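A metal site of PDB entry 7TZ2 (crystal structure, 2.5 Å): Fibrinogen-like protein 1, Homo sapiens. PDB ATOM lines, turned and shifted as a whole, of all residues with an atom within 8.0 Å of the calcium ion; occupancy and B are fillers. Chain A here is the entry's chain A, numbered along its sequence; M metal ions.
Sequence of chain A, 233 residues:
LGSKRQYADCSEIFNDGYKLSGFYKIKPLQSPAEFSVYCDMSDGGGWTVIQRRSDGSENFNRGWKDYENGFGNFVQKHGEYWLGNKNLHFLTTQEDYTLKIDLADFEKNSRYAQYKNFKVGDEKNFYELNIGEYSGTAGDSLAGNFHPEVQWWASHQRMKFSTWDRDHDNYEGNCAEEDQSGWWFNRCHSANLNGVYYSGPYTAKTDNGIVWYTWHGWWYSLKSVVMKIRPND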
ATOM      1  N   SER A 162     -11.298  28.275   8.349  1.00  0.00           N
ATOM      2  CA  SER A 162     -11.425  28.586   9.773  1.00  0.00           C
ATOM      3  C   SER A 162     -10.741  29.910  10.096  1.00  0.00           C
ATOM      4  O   SER A 162      -9.669  30.216   9.561  1.00  0.00           O
ATOM      5  CB  SER A 162     -10.800  27.497  10.671  1.00  0.00           C
ATOM      6  OG  SER A 162     -10.995  26.183  10.162  1.00  0.00           O
ATOM      7  N   ARG A 166     -14.437  31.629  14.085  1.00  0.00           N
ATOM      8  CA  ARG A 166     -15.273  30.568  13.476  1.00  0.00           C
ATOM      9  C   ARG A 166     -14.422  29.312  13.351  1.00  0.00           C
ATOM     10  O   ARG A 166     -13.749  29.165  12.327  1.00  0.00           O
ATOM     11  CB  ARG A 166     -15.813  31.032  12.126  1.00  0.00           C
ATOM     12  CG  ARG A 166     -17.286  31.430  12.129  1.00  0.00           C
ATOM     13  CD  ARG A 166     -17.497  32.811  12.703  1.00  0.00           C
ATOM     14  NE  ARG A 166     -18.730  33.414  12.237  1.00  0.00           N
ATOM     15  CZ  ARG A 166     -19.106  34.649  12.522  1.00  0.00           C
ATOM     16  NH1 ARG A 166     -20.248  35.125  12.043  1.00  0.00           N
ATOM     17  NH2 ARG A 166     -18.338  35.419  13.278  1.00  0.00           N
ATOM     18  N   ASP A 167     -14.464  28.442  14.349  1.00  0.00           N
ATOM     19  CA  ASP A 167     -13.606  27.265  14.369  1.00  0.00           C
ATOM     20  C   ASP A 167     -14.271  26.094  13.646  1.00  0.00           C
ATOM     21  O   ASP A 167     -15.281  25.552  14.130  1.00  0.00           O
ATOM     22  CB  ASP A 167     -13.296  26.873  15.814  1.00  0.00           C
ATOM     23  CG  ASP A 167     -12.259  25.771  15.915  1.00  0.00           C
ATOM     24  OD1 ASP A 167     -11.728  25.358  14.849  1.00  0.00           O
ATOM     25  OD2 ASP A 167     -12.013  25.302  17.039  1.00  0.00           O
ATOM     26  N   HIS A 168     -13.698  25.688  12.511  1.00  0.00           N
ATOM     27  CA  HIS A 168     -14.194  24.530  11.789  1.00  0.00           C
ATOM     28  C   HIS A 168     -13.071  23.535  11.490  1.00  0.00           C
ATOM     29  O   HIS A 168     -13.108  22.851  10.469  1.00  0.00           O
ATOM     30  CB  HIS A 168     -14.860  24.921  10.469  1.00  0.00           C
ATOM     31  CG  HIS A 168     -15.825  26.060  10.574  1.00  0.00           C
ATOM     32  ND1 HIS A 168     -17.073  25.934  11.160  1.00  0.00           N
ATOM     33  CD2 HIS A 168     -15.730  27.348  10.162  1.00  0.00           C
ATOM     34  CE1 HIS A 168     -17.700  27.096  11.104  1.00  0.00           C
ATOM     35  NE2 HIS A 168     -16.903  27.967  10.521  1.00  0.00           N
ATOM     36  N   ASP A 169     -12.092  23.402  12.394  1.00  0.00           N
ATOM     37  CA  ASP A 169     -10.970  22.507  12.137  1.00  0.00           C
ATOM     38  C   ASP A 169     -11.191  21.160  12.812  1.00  0.00           C
ATOM     39  O   ASP A 169     -12.187  20.936  13.507  1.00  0.00           O
ATOM     40  CB  ASP A 169      -9.628  23.157  12.519  1.00  0.00           C
ATOM     41  CG  ASP A 169      -9.559  23.608  13.971  1.00  0.00           C
ATOM     42  OD1 ASP A 169      -9.974  22.852  14.874  1.00  0.00           O
ATOM     43  OD2 ASP A 169      -9.086  24.739  14.208  1.00  0.00           O
ATOM     44  N   ASN A 170     -10.285  20.219  12.555  1.00  0.00           N
ATOM     45  CA  ASN A 170     -10.255  18.932  13.235  1.00  0.00           C
ATOM     46  C   ASN A 170      -9.327  18.913  14.456  1.00  0.00           C
ATOM     47  O   ASN A 170      -8.872  17.831  14.852  1.00  0.00           O
ATOM     48  CB  ASN A 170      -9.855  17.848  12.230  1.00  0.00           C
ATOM     49  CG  ASN A 170     -10.602  17.981  10.932  1.00  0.00           C
ATOM     50  OD1 ASN A 170     -11.794  18.311  10.909  1.00  0.00           O
ATOM     51  ND2 ASN A 170      -9.924  17.688   9.822  1.00  0.00           N
ATOM     52  N   TYR A 171      -9.031  20.065  15.027  1.00  0.00           N
ATOM     53  CA  TYR A 171      -8.199  20.147  16.216  1.00  0.00           C
ATOM     54  C   TYR A 171      -9.049  20.584  17.402  1.00  0.00           C
ATOM     55  O   TYR A 171     -10.108  21.197  17.232  1.00  0.00           O
ATOM     56  CB  TYR A 171      -7.026  21.093  15.960  1.00  0.00           C
ATOM     57  CG  TYR A 171      -6.332  21.670  17.162  1.00  0.00           C
ATOM     58  CD1 TYR A 171      -5.753  20.837  18.130  1.00  0.00           C
ATOM     59  CD2 TYR A 171      -6.192  23.035  17.305  1.00  0.00           C
ATOM     60  CE1 TYR A 171      -5.112  21.364  19.231  1.00  0.00           C
ATOM     61  CE2 TYR A 171      -5.532  23.579  18.388  1.00  0.00           C
ATOM     62  CZ  TYR A 171      -4.999  22.743  19.360  1.00  0.00           C
ATOM     63  OH  TYR A 171      -4.347  23.284  20.448  1.00  0.00           O
ATOM     64  N   GLU A 172      -8.621  20.196  18.615  1.00  0.00           N
ATOM     65  CA  GLU A 172      -9.434  20.469  19.796  1.00  0.00           C
ATOM     66  C   GLU A 172      -9.511  21.961  20.093  1.00  0.00           C
ATOM     67  O   GLU A 172     -10.588  22.479  20.382  1.00  0.00           O
ATOM     68  CB  GLU A 172      -8.899  19.700  20.999  1.00  0.00           C
ATOM     69  CG  GLU A 172      -9.256  18.230  21.001  1.00  0.00           C
ATOM     70  CD  GLU A 172      -8.487  17.415  19.964  1.00  0.00           C
ATOM     71  OE1 GLU A 172      -7.572  17.959  19.303  1.00  0.00           O
ATOM     72  OE2 GLU A 172      -8.823  16.227  19.816  1.00  0.00           O
ATOM     73  N   GLY A 173      -8.363  22.651  20.097  1.00  0.00           N
ATOM     74  CA  GLY A 173      -8.362  24.102  20.208  1.00  0.00           C
ATOM     75  C   GLY A 173      -8.758  24.772  18.905  1.00  0.00           C
ATOM     76  O   GLY A 173      -9.431  24.179  18.055  1.00  0.00           O
ATOM     77  N   ASN A 174      -8.292  26.003  18.726  1.00  0.00           N
ATOM     78  CA  ASN A 174      -8.559  26.790  17.527  1.00  0.00           C
ATOM     79  C   ASN A 174      -7.279  26.924  16.734  1.00  0.00           C
ATOM     80  O   ASN A 174      -6.359  27.644  17.158  1.00  0.00           O
ATOM     81  CB  ASN A 174      -9.098  28.182  17.851  1.00  0.00           C
ATOM     82  CG  ASN A 174     -10.512  28.179  18.385  1.00  0.00           C
ATOM     83  OD1 ASN A 174     -10.900  27.323  19.186  1.00  0.00           O
ATOM     84  ND2 ASN A 174     -11.302  29.153  17.956  1.00  0.00           N
ATOM     85  N   CYS A 175      -7.194  26.231  15.604  1.00  0.00           N
ATOM     86  CA  CYS A 175      -6.006  26.349  14.749  1.00  0.00           C
ATOM     87  C   CYS A 175      -5.772  27.806  14.373  1.00  0.00           C
ATOM     88  O   CYS A 175      -4.634  28.305  14.379  1.00  0.00           O
ATOM     89  CB  CYS A 175      -6.173  25.480  13.494  1.00  0.00           C
ATOM     90  SG  CYS A 175      -5.249  23.906  13.426  1.00  0.00           S
ATOM     91  N   ALA A 176      -6.858  28.500  13.985  1.00  0.00           N
ATOM     92  CA  ALA A 176      -6.749  29.842  13.426  1.00  0.00           C
ATOM     93  C   ALA A 176      -6.405  30.862  14.501  1.00  0.00           C
ATOM     94  O   ALA A 176      -5.801  31.897  14.217  1.00  0.00           O
ATOM     95  CB  ALA A 176      -8.051  30.217  12.739  1.00  0.00           C
ATOM     96  N   ASN A 186      -6.651  21.861   8.944  1.00  0.00           N
ATOM     97  CA  ASN A 186      -6.926  20.484   9.325  1.00  0.00           C
ATOM     98  C   ASN A 186      -6.384  20.308  10.743  1.00  0.00           C
ATOM     99  O   ASN A 186      -7.158  20.252  11.692  1.00  0.00           O
ATOM    100  CB  ASN A 186      -6.257  19.510   8.346  1.00  0.00           C
ATOM    101  CG  ASN A 186      -6.562  18.059   8.650  1.00  0.00           C
ATOM    102  OD1 ASN A 186      -7.288  17.733   9.604  1.00  0.00           O
ATOM    103  ND2 ASN A 186      -6.007  17.174   7.847  1.00  0.00           N
HETATM  104 CA    CA M   1     -11.573  22.954  16.951  1.00  0.00          CA
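Glu 172 touches the calcium ion.
Five residues have an atom within 4 Å of the calcium ion: Asp 167, Asp 169, Tyr 171, Glu 172 and Gly 173.
The nearest printed residue that does not touch the calcium ion is Asn 174 (4.8 Å).
OD1 of Asn 174 sits close to OD2 of Asp 167, 3.2 Å away.
The side-chain carboxylate (OD2) of Asp 169 sits at hydrogen-bond distance from the backbone NH (N) of Cys 175 (2.8 Å).
O of Tyr 171 binds the calcium ion (2.3 Å).
OD2 of Asp 167 is bound to the calcium ion, 2.4 Å away.
The calcium ion is bound by the side-chain carboxylate (OD1) of Asp 169, 2.6 Å away.
The calcium ion is bound by O of Gly 173.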
